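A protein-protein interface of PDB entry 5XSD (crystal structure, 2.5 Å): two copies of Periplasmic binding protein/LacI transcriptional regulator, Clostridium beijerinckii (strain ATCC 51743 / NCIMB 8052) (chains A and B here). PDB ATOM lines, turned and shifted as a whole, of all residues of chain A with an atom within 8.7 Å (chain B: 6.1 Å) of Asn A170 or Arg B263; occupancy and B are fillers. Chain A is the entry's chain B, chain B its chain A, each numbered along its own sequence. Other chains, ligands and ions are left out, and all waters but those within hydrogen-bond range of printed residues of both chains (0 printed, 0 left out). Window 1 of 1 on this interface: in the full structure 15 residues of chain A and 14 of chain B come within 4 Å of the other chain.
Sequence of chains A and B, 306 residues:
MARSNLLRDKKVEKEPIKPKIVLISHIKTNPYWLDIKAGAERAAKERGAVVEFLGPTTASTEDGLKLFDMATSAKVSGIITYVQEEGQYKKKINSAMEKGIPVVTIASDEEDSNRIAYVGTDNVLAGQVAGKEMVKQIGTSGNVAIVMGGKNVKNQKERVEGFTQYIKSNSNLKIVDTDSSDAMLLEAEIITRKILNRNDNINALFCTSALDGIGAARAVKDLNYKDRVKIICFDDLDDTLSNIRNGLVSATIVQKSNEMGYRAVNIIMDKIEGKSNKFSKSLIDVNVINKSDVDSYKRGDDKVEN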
ATOM      1  N   GLN A 128      11.255  -2.807 -34.795  1.00  0.00           N
ATOM      2  CA  GLN A 128      10.406  -2.946 -33.616  1.00  0.00           C
ATOM      3  C   GLN A 128      10.480  -1.713 -32.740  1.00  0.00           C
ATOM      4  O   GLN A 128       9.461  -1.265 -32.238  1.00  0.00           O
ATOM      5  CB  GLN A 128      10.769  -4.187 -32.822  1.00  0.00           C
ATOM      6  CG  GLN A 128      10.760  -5.420 -33.663  1.00  0.00           C
ATOM      7  CD  GLN A 128      11.124  -6.635 -32.877  1.00  0.00           C
ATOM      8  OE1 GLN A 128      11.525  -6.540 -31.716  1.00  0.00           O
ATOM      9  NE2 GLN A 128      10.975  -7.798 -33.495  1.00  0.00           N
ATOM     10  N   GLY A 131       8.267   0.817 -34.289  1.00  0.00           N
ATOM     11  CA  GLY A 131       6.918   0.457 -33.875  1.00  0.00           C
ATOM     12  C   GLY A 131       6.595   0.922 -32.466  1.00  0.00           C
ATOM     13  O   GLY A 131       5.546   1.530 -32.249  1.00  0.00           O
ATOM     14  N   LYS A 132       7.478   0.646 -31.499  1.00  0.00           N
ATOM     15  CA  LYS A 132       7.201   1.046 -30.122  1.00  0.00           C
ATOM     16  C   LYS A 132       7.080   2.547 -30.031  1.00  0.00           C
ATOM     17  O   LYS A 132       6.194   3.090 -29.363  1.00  0.00           O
ATOM     18  CB  LYS A 132       8.276   0.539 -29.151  1.00  0.00           C
ATOM     19  CG  LYS A 132       8.004   0.970 -27.717  1.00  0.00           C
ATOM     20  CD  LYS A 132       9.050   0.490 -26.718  1.00  0.00           C
ATOM     21  CE  LYS A 132       8.915  -1.005 -26.465  1.00  0.00           C
ATOM     22  NZ  LYS A 132      10.039  -1.602 -25.687  1.00  0.00           N
ATOM     23  N   VAL A 135       3.652   3.820 -31.584  1.00  0.00           N
ATOM     24  CA  VAL A 135       2.553   3.609 -30.657  1.00  0.00           C
ATOM     25  C   VAL A 135       2.643   4.616 -29.519  1.00  0.00           C
ATOM     26  O   VAL A 135       1.637   5.145 -29.067  1.00  0.00           O
ATOM     27  CB  VAL A 135       2.522   2.175 -30.118  1.00  0.00           C
ATOM     28  CG1 VAL A 135       1.515   2.048 -28.965  1.00  0.00           C
ATOM     29  CG2 VAL A 135       2.161   1.231 -31.239  1.00  0.00           C
ATOM     30  N   LYS A 136       3.849   4.927 -29.087  1.00  0.00           N
ATOM     31  CA  LYS A 136       4.026   5.959 -28.064  1.00  0.00           C
ATOM     32  C   LYS A 136       3.612   7.342 -28.583  1.00  0.00           C
ATOM     33  O   LYS A 136       3.101   8.174 -27.833  1.00  0.00           O
ATOM     34  CB  LYS A 136       5.478   5.933 -27.577  1.00  0.00           C
ATOM     35  CG  LYS A 136       5.934   7.121 -26.783  1.00  0.00           C
ATOM     36  CD  LYS A 136       7.255   6.809 -26.090  1.00  0.00           C
ATOM     37  CE  LYS A 136       7.804   8.043 -25.397  1.00  0.00           C
ATOM     38  NZ  LYS A 136       8.182   9.075 -26.426  1.00  0.00           N
ATOM     39  N   GLY A 139      -0.653   6.365 -30.174  1.00  0.00           N
ATOM     40  CA  GLY A 139      -1.553   5.440 -29.494  1.00  0.00           C
ATOM     41  C   GLY A 139      -1.711   4.128 -30.229  1.00  0.00           C
ATOM     42  O   GLY A 139      -0.872   3.780 -31.055  1.00  0.00           O
ATOM     43  N   THR A 140      -2.785   3.402 -29.923  1.00  0.00           N
ATOM     44  CA  THR A 140      -2.990   2.053 -30.455  1.00  0.00           C
ATOM     45  C   THR A 140      -4.114   1.912 -31.485  1.00  0.00           C
ATOM     46  O   THR A 140      -4.343   0.814 -32.022  1.00  0.00           O
ATOM     47  CB  THR A 140      -3.264   1.066 -29.310  1.00  0.00           C
ATOM     48  OG1 THR A 140      -4.261   1.614 -28.446  1.00  0.00           O
ATOM     49  CG2 THR A 140      -2.005   0.851 -28.500  1.00  0.00           C
ATOM     50  N   SER A 141      -4.808   3.008 -31.784  1.00  0.00           N
ATOM     51  CA  SER A 141      -5.778   2.969 -32.881  1.00  0.00           C
ATOM     52  C   SER A 141      -5.537   4.103 -33.867  1.00  0.00           C
ATOM     53  O   SER A 141      -5.016   5.168 -33.515  1.00  0.00           O
ATOM     54  CB  SER A 141      -7.232   2.998 -32.360  1.00  0.00           C
ATOM     55  OG  SER A 141      -7.616   4.278 -31.896  1.00  0.00           O
ATOM     56  N   GLY A 162      10.166  -5.910 -38.834  1.00  0.00           N
ATOM     57  CA  GLY A 162      10.174  -5.579 -37.418  1.00  0.00           C
ATOM     58  C   GLY A 162       9.046  -4.637 -37.031  1.00  0.00           C
ATOM     59  O   GLY A 162       8.318  -4.888 -36.074  1.00  0.00           O
ATOM     60  N   PHE A 163       8.909  -3.545 -37.780  1.00  0.00           N
ATOM     61  CA  PHE A 163       7.845  -2.578 -37.553  1.00  0.00           C
ATOM     62  C   PHE A 163       6.469  -3.222 -37.603  1.00  0.00           C
ATOM     63  O   PHE A 163       5.625  -2.966 -36.747  1.00  0.00           O
ATOM     64  CB  PHE A 163       7.913  -1.448 -38.602  1.00  0.00           C
ATOM     65  CG  PHE A 163       6.783  -0.461 -38.499  1.00  0.00           C
ATOM     66  CD1 PHE A 163       6.853   0.595 -37.598  1.00  0.00           C
ATOM     67  CD2 PHE A 163       5.655  -0.579 -39.309  1.00  0.00           C
ATOM     68  CE1 PHE A 163       5.798   1.511 -37.477  1.00  0.00           C
ATOM     69  CE2 PHE A 163       4.583   0.350 -39.206  1.00  0.00           C
ATOM     70  CZ  PHE A 163       4.658   1.388 -38.288  1.00  0.00           C
ATOM     71  N   THR A 164       6.245  -4.051 -38.617  1.00  0.00           N
ATOM     72  CA  THR A 164       4.923  -4.626 -38.853  1.00  0.00           C
ATOM     73  C   THR A 164       4.536  -5.606 -37.756  1.00  0.00           C
ATOM     74  O   THR A 164       3.379  -5.643 -37.320  1.00  0.00           O
ATOM     75  CB  THR A 164       4.858  -5.328 -40.197  1.00  0.00           C
ATOM     76  OG1 THR A 164       5.180  -4.378 -41.219  1.00  0.00           O
ATOM     77  CG2 THR A 164       3.441  -5.911 -40.442  1.00  0.00           C
ATOM     78  N   GLN A 165       5.512  -6.402 -37.330  1.00  0.00           N
ATOM     79  CA  GLN A 165       5.280  -7.400 -36.309  1.00  0.00           C
ATOM     80  C   GLN A 165       4.916  -6.713 -34.999  1.00  0.00           C
ATOM     81  O   GLN A 165       3.989  -7.135 -34.296  1.00  0.00           O
ATOM     82  CB  GLN A 165       6.504  -8.299 -36.101  1.00  0.00           C
ATOM     83  CG  GLN A 165       6.439  -9.093 -34.777  1.00  0.00           C
ATOM     84  CD  GLN A 165       7.133  -8.426 -33.589  1.00  0.00           C
ATOM     85  OE1 GLN A 165       8.125  -7.709 -33.745  1.00  0.00           O
ATOM     86  NE2 GLN A 165       6.590  -8.644 -32.396  1.00  0.00           N
ATOM     87  N   TYR A 166       5.642  -5.652 -34.660  1.00  0.00           N
ATOM     88  CA  TYR A 166       5.365  -4.961 -33.415  1.00  0.00           C
ATOM     89  C   TYR A 166       3.982  -4.335 -33.414  1.00  0.00           C
ATOM     90  O   TYR A 166       3.236  -4.451 -32.430  1.00  0.00           O
ATOM     91  CB  TYR A 166       6.403  -3.893 -33.151  1.00  0.00           C
ATOM     92  CG  TYR A 166       6.220  -3.247 -31.809  1.00  0.00           C
ATOM     93  CD1 TYR A 166       5.314  -2.208 -31.635  1.00  0.00           C
ATOM     94  CD2 TYR A 166       6.943  -3.690 -30.698  1.00  0.00           C
ATOM     95  CE1 TYR A 166       5.123  -1.628 -30.389  1.00  0.00           C
ATOM     96  CE2 TYR A 166       6.766  -3.110 -29.449  1.00  0.00           C
ATOM     97  CZ  TYR A 166       5.852  -2.083 -29.304  1.00  0.00           C
ATOM     98  OH  TYR A 166       5.670  -1.501 -28.075  1.00  0.00           O
ATOM     99  N   ILE A 167       3.663  -3.637 -34.502  1.00  0.00           N
ATOM    100  CA  ILE A 167       2.385  -2.946 -34.622  1.00  0.00           C
ATOM    101  C   ILE A 167       1.221  -3.937 -34.499  1.00  0.00           C
ATOM    102  O   ILE A 167       0.249  -3.707 -33.772  1.00  0.00           O
ATOM    103  CB  ILE A 167       2.275  -2.207 -35.972  1.00  0.00           C
ATOM    104  CG1 ILE A 167       3.273  -1.045 -36.057  1.00  0.00           C
ATOM    105  CG2 ILE A 167       0.862  -1.738 -36.211  1.00  0.00           C
ATOM    106  CD1 ILE A 167       3.074   0.028 -35.023  1.00  0.00           C
ATOM    107  N   LYS A 168       1.341  -5.060 -35.198  1.00  0.00           N
ATOM    108  CA  LYS A 168       0.254  -6.032 -35.244  1.00  0.00           C
ATOM    109  C   LYS A 168       0.044  -6.699 -33.905  1.00  0.00           C
ATOM    110  O   LYS A 168      -1.065  -7.129 -33.595  1.00  0.00           O
ATOM    111  CB  LYS A 168       0.522  -7.095 -36.309  1.00  0.00           C
ATOM    112  CG  LYS A 168       0.242  -6.665 -37.743  1.00  0.00           C
ATOM    113  CD  LYS A 168       0.182  -7.887 -38.660  1.00  0.00           C
ATOM    114  CE  LYS A 168      -0.077  -7.508 -40.114  1.00  0.00           C
ATOM    115  NZ  LYS A 168       0.194  -8.645 -41.044  1.00  0.00           N
ATOM    116  N   SER A 169       1.108  -6.766 -33.112  1.00  0.00           N
ATOM    117  CA  SER A 169       1.085  -7.471 -31.840  1.00  0.00           C
ATOM    118  C   SER A 169       0.762  -6.592 -30.653  1.00  0.00           C
ATOM    119  O   SER A 169       0.433  -7.082 -29.589  1.00  0.00           O
ATOM    120  CB  SER A 169       2.449  -8.124 -31.590  1.00  0.00           C
ATOM    121  OG  SER A 169       2.682  -9.126 -32.554  1.00  0.00           O
ATOM    122  N   ASN A 170       0.855  -5.289 -30.831  1.00  0.00           N
ATOM    123  CA  ASN A 170       0.752  -4.388 -29.693  1.00  0.00           C
ATOM    124  C   ASN A 170      -0.182  -3.227 -29.925  1.00  0.00           C
ATOM    125  O   ASN A 170      -0.135  -2.245 -29.193  1.00  0.00           O
ATOM    126  CB  ASN A 170       2.137  -3.858 -29.328  1.00  0.00           C
ATOM    127  CG  ASN A 170       3.065  -4.958 -28.852  1.00  0.00           C
ATOM    128  OD1 ASN A 170       2.921  -5.443 -27.733  1.00  0.00           O
ATOM    129  ND2 ASN A 170       4.021  -5.354 -29.692  1.00  0.00           N
ATOM    130  N   SER A 171      -1.000  -3.319 -30.972  1.00  0.00           N
ATOM    131  CA  SER A 171      -1.913  -2.240 -31.292  1.00  0.00           C
ATOM    132  C   SER A 171      -2.972  -2.703 -32.268  1.00  0.00           C
ATOM    133  O   SER A 171      -2.894  -3.812 -32.819  1.00  0.00           O
ATOM    134  CB  SER A 171      -1.155  -1.074 -31.903  1.00  0.00           C
ATOM    135  OG  SER A 171      -0.925  -1.359 -33.274  1.00  0.00           O
ATOM    136  N   ASN A 172      -3.949  -1.836 -32.511  1.00  0.00           N
ATOM    137  CA  ASN A 172      -4.910  -2.092 -33.577  1.00  0.00           C
ATOM    138  C   ASN A 172      -4.784  -1.044 -34.694  1.00  0.00           C
ATOM    139  O   ASN A 172      -5.749  -0.744 -35.406  1.00  0.00           O
ATOM    140  CB  ASN A 172      -6.323  -2.119 -33.004  1.00  0.00           C
ATOM    141  CG  ASN A 172      -6.605  -3.391 -32.201  1.00  0.00           C
ATOM    142  OD1 ASN A 172      -6.440  -4.507 -32.696  1.00  0.00           O
ATOM    143  ND2 ASN A 172      -7.011  -3.219 -30.952  1.00  0.00           N
ATOM    144  N   LEU A 173      -3.589  -0.479 -34.826  1.00  0.00           N
ATOM    145  CA  LEU A 173      -3.281   0.466 -35.899  1.00  0.00           C
ATOM    146  C   LEU A 173      -3.384  -0.242 -37.245  1.00  0.00           C
ATOM    147  O   LEU A 173      -2.784  -1.289 -37.425  1.00  0.00           O
ATOM    148  CB  LEU A 173      -1.869   1.040 -35.720  1.00  0.00           C
ATOM    149  CG  LEU A 173      -1.625   1.904 -34.482  1.00  0.00           C
ATOM    150  CD1 LEU A 173      -0.129   2.212 -34.343  1.00  0.00           C
ATOM    151  CD2 LEU A 173      -2.430   3.186 -34.544  1.00  0.00           C
ATOM    152  N   GLY B  39      -6.111  -1.161 -19.718  1.00  0.00           N
ATOM    153  CA  GLY B  39      -5.656  -1.730 -20.971  1.00  0.00           C
ATOM    154  C   GLY B  39      -6.739  -2.594 -21.587  1.00  0.00           C
ATOM    155  O   GLY B  39      -7.012  -2.505 -22.786  1.00  0.00           O
ATOM    156  N   ARG B  42      -9.340  -0.274 -23.026  1.00  0.00           N
ATOM    157  CA  ARG B  42      -8.884   0.366 -24.249  1.00  0.00           C
ATOM    158  C   ARG B  42      -9.001  -0.575 -25.446  1.00  0.00           C
ATOM    159  O   ARG B  42      -9.539  -0.185 -26.496  1.00  0.00           O
ATOM    160  CB  ARG B  42      -7.475   0.903 -24.068  1.00  0.00           C
ATOM    161  CG  ARG B  42      -6.893   1.598 -25.293  1.00  0.00           C
ATOM    162  CD  ARG B  42      -5.736   2.482 -24.862  1.00  0.00           C
ATOM    163  NE  ARG B  42      -4.744   1.757 -24.062  1.00  0.00           N
ATOM    164  CZ  ARG B  42      -3.846   0.907 -24.542  1.00  0.00           C
ATOM    165  NH1 ARG B  42      -3.808   0.659 -25.843  1.00  0.00           N
ATOM    166  NH2 ARG B  42      -2.993   0.305 -23.714  1.00  0.00           N
ATOM    167  N   ALA B  43      -8.537  -1.812 -25.294  1.00  0.00           N
ATOM    168  CA  ALA B  43      -8.699  -2.778 -26.366  1.00  0.00           C
ATOM    169  C   ALA B  43     -10.182  -3.050 -26.656  1.00  0.00           C
ATOM    170  O   ALA B  43     -10.564  -3.231 -27.814  1.00  0.00           O
ATOM    171  CB  ALA B  43      -7.999  -4.063 -26.027  1.00  0.00           C
ATOM    172  N   VAL B 119      -0.927 -14.835 -21.358  1.00  0.00           N
ATOM    173  CA  VAL B 119      -0.358 -13.510 -21.501  1.00  0.00           C
ATOM    174  C   VAL B 119       0.434 -13.204 -20.238  1.00  0.00           C
ATOM    175  O   VAL B 119      -0.115 -13.153 -19.132  1.00  0.00           O
ATOM    176  CB  VAL B 119      -1.422 -12.431 -21.758  1.00  0.00           C
ATOM    177  CG1 VAL B 119      -0.783 -11.029 -21.740  1.00  0.00           C
ATOM    178  CG2 VAL B 119      -2.111 -12.690 -23.084  1.00  0.00           C
ATOM    179  N   ASN B 258      -0.839  -2.789 -17.965  1.00  0.00           N
ATOM    180  CA  ASN B 258      -1.787  -2.240 -18.910  1.00  0.00           C
ATOM    181  C   ASN B 258      -1.800  -3.034 -20.243  1.00  0.00           C
ATOM    182  O   ASN B 258      -2.859  -3.374 -20.781  1.00  0.00           O
ATOM    183  CB  ASN B 258      -1.439  -0.767 -19.136  1.00  0.00           C
ATOM    184  CG  ASN B 258      -2.556   0.014 -19.808  1.00  0.00           C
ATOM    185  OD1 ASN B 258      -2.751  -0.061 -21.021  1.00  0.00           O
ATOM    186  ND2 ASN B 258      -3.288   0.785 -19.012  1.00  0.00           N
ATOM    187  N   GLU B 259      -0.607  -3.368 -20.732  1.00  0.00           N
ATOM    188  CA  GLU B 259      -0.448  -4.030 -22.020  1.00  0.00           C
ATOM    189  C   GLU B 259      -0.896  -5.475 -21.948  1.00  0.00           C
ATOM    190  O   GLU B 259      -1.388  -6.028 -22.928  1.00  0.00           O
ATOM    191  CB  GLU B 259       1.022  -3.934 -22.517  1.00  0.00           C
ATOM    192  CG  GLU B 259       1.669  -2.498 -22.513  1.00  0.00           C
ATOM    193  CD  GLU B 259       1.749  -1.779 -21.129  1.00  0.00           C
ATOM    194  OE1 GLU B 259       1.189  -2.268 -20.120  1.00  0.00           O
ATOM    195  OE2 GLU B 259       2.388  -0.704 -21.052  1.00  0.00           O
ATOM    196  N   MET B 260      -0.763  -6.079 -20.776  1.00  0.00           N
ATOM    197  CA  MET B 260      -1.177  -7.466 -20.614  1.00  0.00           C
ATOM    198  C   MET B 260      -2.692  -7.562 -20.761  1.00  0.00           C
ATOM    199  O   MET B 260      -3.209  -8.443 -21.462  1.00  0.00           O
ATOM    200  CB  MET B 260      -0.737  -8.004 -19.252  1.00  0.00           C
ATOM    201  CG  MET B 260       0.781  -8.120 -19.081  1.00  0.00           C
ATOM    202  SD  MET B 260       1.208  -8.793 -17.448  1.00  0.00           S
ATOM    203  CE  MET B 260       0.247 -10.291 -17.462  1.00  0.00           C
ATOM    204  N   GLY B 261      -3.392  -6.621 -20.131  1.00  0.00           N
ATOM    205  CA  GLY B 261      -4.837  -6.556 -20.216  1.00  0.00           C
ATOM    206  C   GLY B 261      -5.262  -6.193 -21.626  1.00  0.00           C
ATOM    207  O   GLY B 261      -6.210  -6.761 -22.171  1.00  0.00           O
ATOM    208  N   TYR B 262      -4.543  -5.248 -22.221  1.00  0.00           N
ATOM    209  CA  TYR B 262      -4.812  -4.846 -23.591  1.00  0.00           C
ATOM    210  C   TYR B 262      -4.659  -6.062 -24.513  1.00  0.00           C
ATOM    211  O   TYR B 262      -5.574  -6.400 -25.274  1.00  0.00           O
ATOM    212  CB  TYR B 262      -3.874  -3.686 -24.001  1.00  0.00           C
ATOM    213  CG  TYR B 262      -4.076  -3.216 -25.422  1.00  0.00           C
ATOM    214  CD1 TYR B 262      -5.063  -2.298 -25.732  1.00  0.00           C
ATOM    215  CD2 TYR B 262      -3.270  -3.694 -26.458  1.00  0.00           C
ATOM    216  CE1 TYR B 262      -5.259  -1.871 -27.029  1.00  0.00           C
ATOM    217  CE2 TYR B 262      -3.452  -3.269 -27.766  1.00  0.00           C
ATOM    218  CZ  TYR B 262      -4.455  -2.355 -28.041  1.00  0.00           C
ATOM    219  OH  TYR B 262      -4.668  -1.925 -29.330  1.00  0.00           O
ATOM    220  N   ARG B 263      -3.529  -6.758 -24.403  1.00  0.00           N
ATOM    221  CA  ARG B 263      -3.293  -7.932 -25.235  1.00  0.00           C
ATOM    222  C   ARG B 263      -4.314  -9.055 -25.027  1.00  0.00           C
ATOM    223  O   ARG B 263      -4.720  -9.708 -25.988  1.00  0.00           O
ATOM    224  CB  ARG B 263      -1.890  -8.485 -24.986  1.00  0.00           C
ATOM    225  CG  ARG B 263      -1.659  -9.838 -25.661  1.00  0.00           C
ATOM    226  CD  ARG B 263      -1.252  -9.660 -27.099  1.00  0.00           C
ATOM    227  NE  ARG B 263      -0.165  -8.696 -27.185  1.00  0.00           N
ATOM    228  CZ  ARG B 263       1.119  -9.022 -27.285  1.00  0.00           C
ATOM    229  NH1 ARG B 263       1.477 -10.298 -27.336  1.00  0.00           N
ATOM    230  NH2 ARG B 263       2.040  -8.069 -27.348  1.00  0.00           N
ATOM    231  N   ALA B 264      -4.737  -9.266 -23.783  1.00  0.00           N
ATOM    232  CA  ALA B 264      -5.631 -10.375 -23.460  1.00  0.00           C
ATOM    233  C   ALA B 264      -6.954 -10.218 -24.196  1.00  0.00           C
ATOM    234  O   ALA B 264      -7.452 -11.155 -24.809  1.00  0.00           O
ATOM    235  CB  ALA B 264      -5.858 -10.463 -21.938  1.00  0.00           C
ATOM    236  N   VAL B 265      -7.521  -9.022 -24.123  1.00  0.00           N
ATOM    237  CA  VAL B 265      -8.735  -8.719 -24.852  1.00  0.00           C
ATOM    238  C   VAL B 265      -8.587  -8.952 -26.366  1.00  0.00           C
ATOM    239  O   VAL B 265      -9.419  -9.633 -26.970  1.00  0.00           O
ATOM    240  CB  VAL B 265      -9.153  -7.279 -24.612  1.00  0.00           C
ATOM    241  CG1 VAL B 265     -10.343  -6.934 -25.491  1.00  0.00           C
ATOM    242  CG2 VAL B 265      -9.459  -7.063 -23.140  1.00  0.00           C
ATOM    243  N   ASN B 266      -7.524  -8.413 -26.969  1.00  0.00           N
ATOM    244  CA  ASN B 266      -7.318  -8.588 -28.409  1.00  0.00           C
ATOM    245  C   ASN B 266      -7.170 -10.051 -28.793  1.00  0.00           C
ATOM    246  O   ASN B 266      -7.586 -10.454 -29.876  1.00  0.00           O
ATOM    247  CB  ASN B 266      -6.107  -7.775 -28.907  1.00  0.00           C
ATOM    248  CG  ASN B 266      -6.468  -6.308 -29.153  1.00  0.00           C
ATOM    249  OD1 ASN B 266      -7.463  -6.007 -29.821  1.00  0.00           O
ATOM    250  ND2 ASN B 266      -5.678  -5.398 -28.607  1.00  0.00           N
ATOM    251  N   ILE B 267      -6.624 -10.858 -27.892  1.00  0.00           N
ATOM    252  CA  ILE B 267      -6.524 -12.293 -28.141  1.00  0.00           C
ATOM    253  C   ILE B 267      -7.887 -12.988 -28.081  1.00  0.00           C
ATOM    254  O   ILE B 267      -8.205 -13.812 -28.938  1.00  0.00           O
ATOM    255  CB  ILE B 267      -5.577 -12.953 -27.155  1.00  0.00           C
ATOM    256  CG1 ILE B 267      -4.140 -12.503 -27.461  1.00  0.00           C
ATOM    257  CG2 ILE B 267      -5.688 -14.462 -27.249  1.00  0.00           C
ATOM    258  CD1 ILE B 267      -3.081 -13.179 -26.607  1.00  0.00           C
ATOM    259  N   ILE B 268      -8.701 -12.624 -27.096  1.00  0.00           N
ATOM    260  CA  ILE B 268     -10.071 -13.134 -26.998  1.00  0.00           C
ATOM    261  C   ILE B 268     -10.869 -12.813 -28.257  1.00  0.00           C
ATOM    262  O   ILE B 268     -11.454 -13.694 -28.890  1.00  0.00           O
ATOM    263  CB  ILE B 268     -10.809 -12.537 -25.791  1.00  0.00           C
ATOM    264  CG1 ILE B 268     -10.197 -13.052 -24.499  1.00  0.00           C
ATOM    265  CG2 ILE B 268     -12.278 -12.882 -25.851  1.00  0.00           C
ATOM    266  CD1 ILE B 268     -10.546 -14.503 -24.222  1.00  0.00           C
ATOM    267  N   LYS B 281       3.141 -18.601 -27.539  1.00  0.00           N
ATOM    268  CA  LYS B 281       2.252 -17.762 -26.736  1.00  0.00           C
ATOM    269  C   LYS B 281       2.440 -16.286 -27.105  1.00  0.00           C
ATOM    270  O   LYS B 281       2.731 -15.946 -28.261  1.00  0.00           O
ATOM    271  CB  LYS B 281       2.499 -17.977 -25.233  1.00  0.00           C
ATOM    272  CG  LYS B 281       2.211 -19.394 -24.745  1.00  0.00           C
ATOM    273  CD  LYS B 281       3.369 -19.909 -23.897  1.00  0.00           C
ATOM    274  CE  LYS B 281       3.076 -21.265 -23.255  1.00  0.00           C
ATOM    275  NZ  LYS B 281       3.951 -21.487 -22.066  1.00  0.00           N
ATOM    276  N   SER B 282       2.269 -15.408 -26.126  1.00  0.00           N
ATOM    277  CA  SER B 282       2.442 -13.984 -26.380  1.00  0.00           C
ATOM    278  C   SER B 282       2.960 -13.299 -25.120  1.00  0.00           C
ATOM    279  O   SER B 282       2.191 -12.966 -24.209  1.00  0.00           O
ATOM    280  CB  SER B 282       1.133 -13.343 -26.845  1.00  0.00           C
ATOM    281  OG  SER B 282       0.194 -13.326 -25.794  1.00  0.00           O
ATOM    282  N   LEU B 283       4.278 -13.119 -25.089  1.00  0.00           N
ATOM    283  CA  LEU B 283       4.966 -12.568 -23.937  1.00  0.00           C
ATOM    284  C   LEU B 283       5.094 -11.065 -24.054  1.00  0.00           C
ATOM    285  O   LEU B 283       5.287 -10.553 -25.146  1.00  0.00           O
ATOM    286  CB  LEU B 283       6.338 -13.205 -23.812  1.00  0.00           C
ATOM    287  CG  LEU B 283       6.269 -14.729 -23.734  1.00  0.00           C
ATOM    288  CD1 LEU B 283       7.674 -15.301 -23.582  1.00  0.00           C
ATOM    289  CD2 LEU B 283       5.300 -15.224 -22.616  1.00  0.00           C
ATOM    290  N   ILE B 284       5.029 -10.366 -22.923  1.00  0.00           N
ATOM    291  CA  ILE B 284       5.011  -8.905 -22.922  1.00  0.00           C
ATOM    292  C   ILE B 284       6.367  -8.328 -22.490  1.00  0.00           C
ATOM    293  O   ILE B 284       7.120  -8.952 -21.734  1.00  0.00           O
ATOM    294  CB  ILE B 284       3.893  -8.379 -22.005  1.00  0.00           C
ATOM    295  CG1 ILE B 284       2.570  -9.018 -22.395  1.00  0.00           C
ATOM    296  CG2 ILE B 284       3.745  -6.875 -22.097  1.00  0.00           C
ATOM    297  CD1 ILE B 284       2.234  -8.803 -23.827  1.00  0.00           C
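NH1 of Arg B42 lies within hydrogen-bond range of OG1 of Thr A140. The side-chain hydroxyl (OH) of Tyr B262 sits at hydrogen-bond distance from the side-chain amide nitrogen (ND2) of Asn A172, 3.1 Å away. The backbone carbonyl oxygen of Ser A169 sits at hydrogen-bond distance from the guanidinium group of Arg B263. The guanidinium group (NH2) of Arg B263 sits at hydrogen-bond distance from the side-chain amide oxygen (OD1) of Asn A170 (2.8 Å). ND2 of Asn A172 is in hydrogen-bond range of OD1 of Asn B266 (3.0 Å).
ND2 of Asn B266 lies close to O of Tyr B262 (3.5 Å). The backbone NH (N) of Asn A172 sits at hydrogen-bond distance from the backbone carbonyl oxygen (O) of Thr A140 (2.7 Å). O of Thr A140 lies within hydrogen-bond range of N of Leu A173 (3.2 Å). The backbone carbonyl oxygen (O) of Gln A165 is in hydrogen-bond range of the side-chain hydroxyl (OG) of Ser A169, 3.0 Å away. The backbone carbonyl oxygen (O) of Tyr A166 lies within hydrogen-bond range of the side-chain amide nitrogen (ND2) of Asn A170 (3.0 Å). The backbone NH (N) of Leu A173 sits at hydrogen-bond distance from the side-chain hydroxyl (OG) of Ser A171.
Among the printed residues, pairs that only touch across the chains: Thr A140 with Tyr B262 (3.3 Å), Asn A170 with Tyr B262 (3.8 Å) and Ser A171 with Tyr B262 (3.4 Å).
Asn A170 touches just these residues of chain B: Tyr B262 (3.8 Å) and Arg B263 (2.8 Å). Of chain A, only Ser A169 (2.9 Å) and Asn A170 (2.8 Å) come within 4 Å of Arg B263. Of the printed residues of chain B, Asn A172 touches Tyr B262 (3.1 Å) and Asn B266 (3.0 Å). Of the printed residues of chain A, Arg B42 touches Thr A140 (2.8 Å). Of the printed residues of chain B, Ser A171 touches Tyr B262 (3.4 Å). Val B119 touches none of the printed residues of chain A. The nearest residue of chain A that does not touch Arg B263 is Tyr A166 (6.4 Å). The nearest printed residue of chain B that does not touch Thr A140 is Ala B43 (6.3 Å).
Of the 20 printed residues of chain A, 5 touch a printed residue of chain B. Of the 19 printed residues of chain B, 4 touch a printed residue of chain A. Hydrophobic or aromatic side chains of chain B within 4 Å of the printed part of chain A: Tyr B262. Along chain B the printed residues that touch a printed residue of chain A span positions 42 to 266. Among the printed residues, no Asp or Glu carboxylate lies within 4 Å of a Lys or Arg side-chain nitrogen of the other chain.
No position is printed for both chains. Of the 8 pairs that touch across the chains among the printed residues, none has its exchanged pair printed and touching as well.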
